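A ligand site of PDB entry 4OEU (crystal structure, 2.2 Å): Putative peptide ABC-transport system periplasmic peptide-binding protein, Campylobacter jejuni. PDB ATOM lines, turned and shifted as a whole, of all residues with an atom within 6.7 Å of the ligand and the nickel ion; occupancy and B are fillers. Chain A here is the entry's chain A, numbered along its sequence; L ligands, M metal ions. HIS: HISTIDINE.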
ATOM      1  N   ASN A  13      27.989  21.513   4.338  1.00  0.00           N
ATOM      2  CA  ASN A  13      28.395  20.774   3.144  1.00  0.00           C
ATOM      3  C   ASN A  13      29.755  20.107   3.304  1.00  0.00           C
ATOM      4  O   ASN A  13      30.698  20.702   3.838  1.00  0.00           O
ATOM      5  CB  ASN A  13      28.420  21.689   1.913  1.00  0.00           C
ATOM      6  CG  ASN A  13      27.045  21.918   1.330  1.00  0.00           C
ATOM      7  OD1 ASN A  13      26.361  22.877   1.680  1.00  0.00           O
ATOM      8  ND2 ASN A  13      26.614  21.008   0.454  1.00  0.00           N
ATOM      9  N   GLU A  24      34.090  23.145  -5.596  1.00  0.00           N
ATOM     10  CA  GLU A  24      32.819  23.537  -6.164  1.00  0.00           C
ATOM     11  C   GLU A  24      32.176  24.627  -5.324  1.00  0.00           C
ATOM     12  O   GLU A  24      30.959  24.748  -5.289  1.00  0.00           O
ATOM     13  CB  GLU A  24      31.906  22.325  -6.262  1.00  0.00           C
ATOM     14  CG  GLU A  24      32.374  21.283  -7.241  1.00  0.00           C
ATOM     15  CD  GLU A  24      31.582  20.000  -7.143  1.00  0.00           C
ATOM     16  OE1 GLU A  24      30.951  19.765  -6.091  1.00  0.00           O
ATOM     17  OE2 GLU A  24      31.585  19.213  -8.116  1.00  0.00           O
ATOM     18  N   ASP A  25      33.013  25.390  -4.616  1.00  0.00           N
ATOM     19  CA  ASP A  25      32.545  26.461  -3.734  1.00  0.00           C
ATOM     20  C   ASP A  25      31.485  25.970  -2.737  1.00  0.00           C
ATOM     21  O   ASP A  25      30.592  26.729  -2.350  1.00  0.00           O
ATOM     22  CB  ASP A  25      31.994  27.623  -4.550  1.00  0.00           C
ATOM     23  CG  ASP A  25      33.065  28.337  -5.354  1.00  0.00           C
ATOM     24  OD1 ASP A  25      34.241  28.304  -4.938  1.00  0.00           O
ATOM     25  OD2 ASP A  25      32.713  28.937  -6.392  1.00  0.00           O
ATOM     26  N   HIS A  26      31.578  24.715  -2.329  1.00  0.00           N
ATOM     27  CA  HIS A  26      30.621  24.150  -1.396  1.00  0.00           C
ATOM     28  C   HIS A  26      31.303  23.557  -0.180  1.00  0.00           C
ATOM     29  O   HIS A  26      30.807  22.602   0.401  1.00  0.00           O
ATOM     30  CB  HIS A  26      29.771  23.064  -2.070  1.00  0.00           C
ATOM     31  CG  HIS A  26      28.564  23.580  -2.791  1.00  0.00           C
ATOM     32  ND1 HIS A  26      28.648  24.215  -4.015  1.00  0.00           N
ATOM     33  CD2 HIS A  26      27.256  23.550  -2.469  1.00  0.00           C
ATOM     34  CE1 HIS A  26      27.433  24.551  -4.417  1.00  0.00           C
ATOM     35  NE2 HIS A  26      26.565  24.168  -3.488  1.00  0.00           N
ATOM     36  N   ASP A 240      24.652  35.038  -1.917  1.00  0.00           N
ATOM     37  CA  ASP A 240      23.820  33.841  -2.057  1.00  0.00           C
ATOM     38  C   ASP A 240      22.370  34.202  -2.322  1.00  0.00           C
ATOM     39  O   ASP A 240      21.772  34.994  -1.587  1.00  0.00           O
ATOM     40  CB  ASP A 240      23.911  32.979  -0.797  1.00  0.00           C
ATOM     41  CG  ASP A 240      23.367  31.575  -1.009  1.00  0.00           C
ATOM     42  OD1 ASP A 240      23.103  31.187  -2.170  1.00  0.00           O
ATOM     43  OD2 ASP A 240      23.205  30.858  -0.005  1.00  0.00           O
ATOM     44  N   ARG A 242      18.343  32.516  -3.404  1.00  0.00           N
ATOM     45  CA  ARG A 242      17.516  31.326  -3.573  1.00  0.00           C
ATOM     46  C   ARG A 242      16.603  31.568  -4.765  1.00  0.00           C
ATOM     47  O   ARG A 242      16.227  32.700  -5.055  1.00  0.00           O
ATOM     48  CB  ARG A 242      16.685  31.016  -2.308  1.00  0.00           C
ATOM     49  CG  ARG A 242      17.526  30.651  -1.101  1.00  0.00           C
ATOM     50  CD  ARG A 242      18.068  29.224  -1.210  1.00  0.00           C
ATOM     51  NE  ARG A 242      19.155  28.995  -0.252  1.00  0.00           N
ATOM     52  CZ  ARG A 242      20.406  29.376  -0.467  1.00  0.00           C
ATOM     53  NH1 ARG A 242      20.726  29.980  -1.597  1.00  0.00           N
ATOM     54  NH2 ARG A 242      21.345  29.133   0.445  1.00  0.00           N
ATOM     55  N   MET A 338      15.315  20.507  -0.456  1.00  0.00           N
ATOM     56  CA  MET A 338      16.133  19.771   0.493  1.00  0.00           C
ATOM     57  C   MET A 338      15.490  19.890   1.875  1.00  0.00           C
ATOM     58  O   MET A 338      15.404  20.983   2.451  1.00  0.00           O
ATOM     59  CB  MET A 338      17.574  20.289   0.494  1.00  0.00           C
ATOM     60  CG  MET A 338      18.243  20.154  -0.877  1.00  0.00           C
ATOM     61  SD  MET A 338      19.927  20.824  -0.973  1.00  0.00           S
ATOM     62  CE  MET A 338      19.776  22.245   0.106  1.00  0.00           C
ATOM     63  N   ARG A 344      14.279  26.412   2.463  1.00  0.00           N
ATOM     64  CA  ARG A 344      13.896  25.891   1.156  1.00  0.00           C
ATOM     65  C   ARG A 344      12.538  25.191   1.173  1.00  0.00           C
ATOM     66  O   ARG A 344      11.744  25.370   0.252  1.00  0.00           O
ATOM     67  CB  ARG A 344      14.975  24.962   0.611  1.00  0.00           C
ATOM     68  CG  ARG A 344      16.360  25.590   0.610  1.00  0.00           C
ATOM     69  CD  ARG A 344      17.190  25.059  -0.542  1.00  0.00           C
ATOM     70  NE  ARG A 344      18.597  25.434  -0.408  1.00  0.00           N
ATOM     71  CZ  ARG A 344      19.492  25.336  -1.382  1.00  0.00           C
ATOM     72  NH1 ARG A 344      20.759  25.697  -1.154  1.00  0.00           N
ATOM     73  NH2 ARG A 344      19.134  24.903  -2.575  1.00  0.00           N
ATOM     74  N   ALA A 369      19.189  16.441   1.305  1.00  0.00           N
ATOM     75  CA  ALA A 369      20.217  16.725   0.307  1.00  0.00           C
ATOM     76  C   ALA A 369      21.083  15.488   0.086  1.00  0.00           C
ATOM     77  O   ALA A 369      21.457  14.805   1.042  1.00  0.00           O
ATOM     78  CB  ALA A 369      21.080  17.912   0.747  1.00  0.00           C
ATOM     79  N   GLY A 370      21.350  15.181  -1.174  1.00  0.00           N
ATOM     80  CA  GLY A 370      22.133  14.002  -1.522  1.00  0.00           C
ATOM     81  C   GLY A 370      21.320  12.742  -1.772  1.00  0.00           C
ATOM     82  O   GLY A 370      21.857  11.754  -2.256  1.00  0.00           O
ATOM     83  N   TYR A 374      18.796  16.322  -8.443  1.00  0.00           N
ATOM     84  CA  TYR A 374      17.989  17.512  -8.679  1.00  0.00           C
ATOM     85  C   TYR A 374      18.025  17.972 -10.142  1.00  0.00           C
ATOM     86  O   TYR A 374      17.249  18.859 -10.531  1.00  0.00           O
ATOM     87  CB  TYR A 374      18.417  18.660  -7.757  1.00  0.00           C
ATOM     88  CG  TYR A 374      19.890  18.759  -7.528  1.00  0.00           C
ATOM     89  CD1 TYR A 374      20.696  19.461  -8.413  1.00  0.00           C
ATOM     90  CD2 TYR A 374      20.488  18.157  -6.428  1.00  0.00           C
ATOM     91  CE1 TYR A 374      22.060  19.557  -8.207  1.00  0.00           C
ATOM     92  CE2 TYR A 374      21.850  18.251  -6.213  1.00  0.00           C
ATOM     93  CZ  TYR A 374      22.628  18.960  -7.112  1.00  0.00           C
ATOM     94  OH  TYR A 374      23.987  19.072  -6.924  1.00  0.00           O
ATOM     95  N   PHE A 380      13.245  22.719  -8.860  1.00  0.00           N
ATOM     96  CA  PHE A 380      14.099  22.534  -7.695  1.00  0.00           C
ATOM     97  C   PHE A 380      14.389  23.854  -7.019  1.00  0.00           C
ATOM     98  O   PHE A 380      14.709  24.850  -7.678  1.00  0.00           O
ATOM     99  CB  PHE A 380      15.409  21.841  -8.125  1.00  0.00           C
ATOM    100  CG  PHE A 380      16.434  21.692  -7.031  1.00  0.00           C
ATOM    101  CD1 PHE A 380      16.239  20.814  -5.974  1.00  0.00           C
ATOM    102  CD2 PHE A 380      17.646  22.380  -7.104  1.00  0.00           C
ATOM    103  CE1 PHE A 380      17.207  20.648  -4.981  1.00  0.00           C
ATOM    104  CE2 PHE A 380      18.616  22.217  -6.121  1.00  0.00           C
ATOM    105  CZ  PHE A 380      18.394  21.363  -5.062  1.00  0.00           C
ATOM    106  N   LEU A 381      14.227  23.892  -5.707  1.00  0.00           N
ATOM    107  CA  LEU A 381      14.548  25.106  -5.001  1.00  0.00           C
ATOM    108  C   LEU A 381      16.071  25.215  -4.822  1.00  0.00           C
ATOM    109  O   LEU A 381      16.662  24.645  -3.895  1.00  0.00           O
ATOM    110  CB  LEU A 381      13.843  25.171  -3.668  1.00  0.00           C
ATOM    111  CG  LEU A 381      13.543  26.642  -3.433  1.00  0.00           C
ATOM    112  CD1 LEU A 381      12.416  27.134  -4.345  1.00  0.00           C
ATOM    113  CD2 LEU A 381      13.182  26.819  -2.028  1.00  0.00           C
ATOM    114  N   ILE A 382      16.675  25.993  -5.717  1.00  0.00           N
ATOM    115  CA  ILE A 382      18.104  26.014  -5.910  1.00  0.00           C
ATOM    116  C   ILE A 382      18.715  27.249  -5.266  1.00  0.00           C
ATOM    117  O   ILE A 382      17.987  28.153  -4.824  1.00  0.00           O
ATOM    118  CB  ILE A 382      18.444  25.994  -7.413  1.00  0.00           C
ATOM    119  CG1 ILE A 382      19.860  25.456  -7.661  1.00  0.00           C
ATOM    120  CG2 ILE A 382      18.269  27.379  -8.014  1.00  0.00           C
ATOM    121  CD1 ILE A 382      20.074  24.971  -9.078  1.00  0.00           C
ATOM    122  N   GLY A 383      20.043  27.258  -5.177  1.00  0.00           N
ATOM    123  CA  GLY A 383      20.794  28.415  -4.704  1.00  0.00           C
ATOM    124  C   GLY A 383      22.164  28.495  -5.350  1.00  0.00           C
ATOM    125  O   GLY A 383      22.789  27.476  -5.654  1.00  0.00           O
ATOM    126  N   TRP A 384      22.638  29.726  -5.550  1.00  0.00           N
ATOM    127  CA  TRP A 384      23.983  30.015  -6.046  1.00  0.00           C
ATOM    128  C   TRP A 384      24.421  31.396  -5.587  1.00  0.00           C
ATOM    129  O   TRP A 384      23.625  32.139  -5.004  1.00  0.00           O
ATOM    130  CB  TRP A 384      24.029  29.982  -7.583  1.00  0.00           C
ATOM    131  CG  TRP A 384      23.782  28.647  -8.222  1.00  0.00           C
ATOM    132  CD1 TRP A 384      22.690  28.281  -8.945  1.00  0.00           C
ATOM    133  CD2 TRP A 384      24.660  27.522  -8.228  1.00  0.00           C
ATOM    134  NE1 TRP A 384      22.828  26.987  -9.398  1.00  0.00           N
ATOM    135  CE2 TRP A 384      24.025  26.497  -8.968  1.00  0.00           C
ATOM    136  CE3 TRP A 384      25.924  27.271  -7.675  1.00  0.00           C
ATOM    137  CZ2 TRP A 384      24.606  25.238  -9.159  1.00  0.00           C
ATOM    138  CZ3 TRP A 384      26.497  26.016  -7.877  1.00  0.00           C
ATOM    139  CH2 TRP A 384      25.836  25.024  -8.613  1.00  0.00           C
ATOM    140  N   PHE A 413      21.957  22.617 -14.127  1.00  0.00           N
ATOM    141  CA  PHE A 413      21.170  21.456 -13.707  1.00  0.00           C
ATOM    142  C   PHE A 413      19.767  21.441 -14.343  1.00  0.00           C
ATOM    143  O   PHE A 413      19.122  20.396 -14.423  1.00  0.00           O
ATOM    144  CB  PHE A 413      21.079  21.390 -12.176  1.00  0.00           C
ATOM    145  CG  PHE A 413      22.406  21.165 -11.486  1.00  0.00           C
ATOM    146  CD1 PHE A 413      23.272  20.163 -11.926  1.00  0.00           C
ATOM    147  CD2 PHE A 413      22.809  21.959 -10.426  1.00  0.00           C
ATOM    148  CE1 PHE A 413      24.507  19.944 -11.296  1.00  0.00           C
ATOM    149  CE2 PHE A 413      24.038  21.753  -9.803  1.00  0.00           C
ATOM    150  CZ  PHE A 413      24.891  20.740 -10.239  1.00  0.00           C
ATOM    151  N   HIS A 480      27.847  31.427  -1.642  1.00  0.00           N
ATOM    152  CA  HIS A 480      26.788  30.435  -1.591  1.00  0.00           C
ATOM    153  C   HIS A 480      26.947  29.488  -0.384  1.00  0.00           C
ATOM    154  O   HIS A 480      28.048  29.018  -0.095  1.00  0.00           O
ATOM    155  CB  HIS A 480      26.782  29.663  -2.923  1.00  0.00           C
ATOM    156  CG  HIS A 480      25.781  28.570  -3.005  1.00  0.00           C
ATOM    157  ND1 HIS A 480      24.455  28.732  -2.653  1.00  0.00           N
ATOM    158  CD2 HIS A 480      25.887  27.285  -3.440  1.00  0.00           C
ATOM    159  CE1 HIS A 480      23.806  27.605  -2.842  1.00  0.00           C
ATOM    160  NE2 HIS A 480      24.645  26.714  -3.330  1.00  0.00           N
ATOM    161  N   HIS A 481      25.840  29.247   0.324  1.00  0.00           N
ATOM    162  CA  HIS A 481      25.801  28.463   1.578  1.00  0.00           C
ATOM    163  C   HIS A 481      26.571  29.132   2.722  1.00  0.00           C
ATOM    164  O   HIS A 481      26.788  28.523   3.762  1.00  0.00           O
ATOM    165  CB  HIS A 481      26.367  27.046   1.393  1.00  0.00           C
ATOM    166  CG  HIS A 481      25.553  26.166   0.509  1.00  0.00           C
ATOM    167  ND1 HIS A 481      24.320  25.655   0.870  1.00  0.00           N
ATOM    168  CD2 HIS A 481      25.802  25.690  -0.739  1.00  0.00           C
ATOM    169  CE1 HIS A 481      23.856  24.895  -0.108  1.00  0.00           C
ATOM    170  NE2 HIS A 481      24.730  24.908  -1.098  1.00  0.00           N
HETATM  171  N   HIS L   1      24.360  24.787  -5.194  1.00  0.00           N
HETATM  172  CA  HIS L   1      23.034  24.263  -5.523  1.00  0.00           C
HETATM  173  C   HIS L   1      22.030  24.627  -4.454  1.00  0.00           C
HETATM  174  O   HIS L   1      22.425  25.048  -3.373  1.00  0.00           O
HETATM  175  CB  HIS L   1      23.096  22.736  -5.664  1.00  0.00           C
HETATM  176  CG  HIS L   1      23.391  22.025  -4.383  1.00  0.00           C
HETATM  177  ND1 HIS L   1      24.208  22.558  -3.395  1.00  0.00           N
HETATM  178  CD2 HIS L   1      22.997  20.818  -3.905  1.00  0.00           C
HETATM  179  CE1 HIS L   1      24.295  21.722  -2.393  1.00  0.00           C
HETATM  180  NE2 HIS L   1      23.566  20.659  -2.665  1.00  0.00           N
HETATM  181  OXT HIS L   1      20.814  24.481  -4.611  1.00  0.00           O
HETATM  182 NI    NI M   1      24.602  24.635  -3.278  1.00  0.00          NI
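Within 4 Å of the nickel ion: His 26, His 480 and His 481.
The nearest printed residue that does not touch the nickel ion is Gly 383 (4.1 Å).
An oxygen (OXT) of the ligand lies within salt-bridge range of the guanidinium group (NH2) of Arg 344.
An oxygen (OXT) of the ligand lies within hydrogen-bond range of the backbone NH (N) of Gly 383, 2.9 Å away.
N of the ligand sits close to O of Gly 383, 3.1 Å away.
A ring nitrogen (ND1) of His 26 sits at hydrogen-bond distance from the backbone carbonyl oxygen (O) of Glu 24.
NE2 of His 480 sits close to O of Gly 383, at 3.1 Å.
A ring nitrogen (ND1) of His 480 lies within hydrogen-bond range of the side-chain carboxylate (OD1) of Asp 240, 2.8 Å away.
N of His 481 sits at hydrogen-bond distance from OD2 of Asp 240.
The guanidinium group (NH2) of Arg 344 sits at hydrogen-bond distance from the backbone carbonyl oxygen (O) of Leu 381 (2.8 Å).
Merely in contact with the ligand: Ile 382, Phe 380, Tyr 374, Trp 384 and Asn 13.
Hydrophobic or aromatic side chains within 4 Å of the ligand: His 26, Tyr 374, Phe 380, Ile 382, Trp 384, His 480 and His 481.
The nearest printed residue that does not touch the ligand is Met 338 (4.02 Å).
The nickel ion is bound by a nitrogen (N) of the ligand (1.9 Å), a ring nitrogen (NE2) of His 26 (2.0 Å), a ring nitrogen (NE2) of His 480 (2.1 Å), a nitrogen (ND1) of the ligand (2.1 Å), a ring nitrogen (NE2) of His 481 (2.2 Å) and an oxygen (O) of the ligand (2.2 Å).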
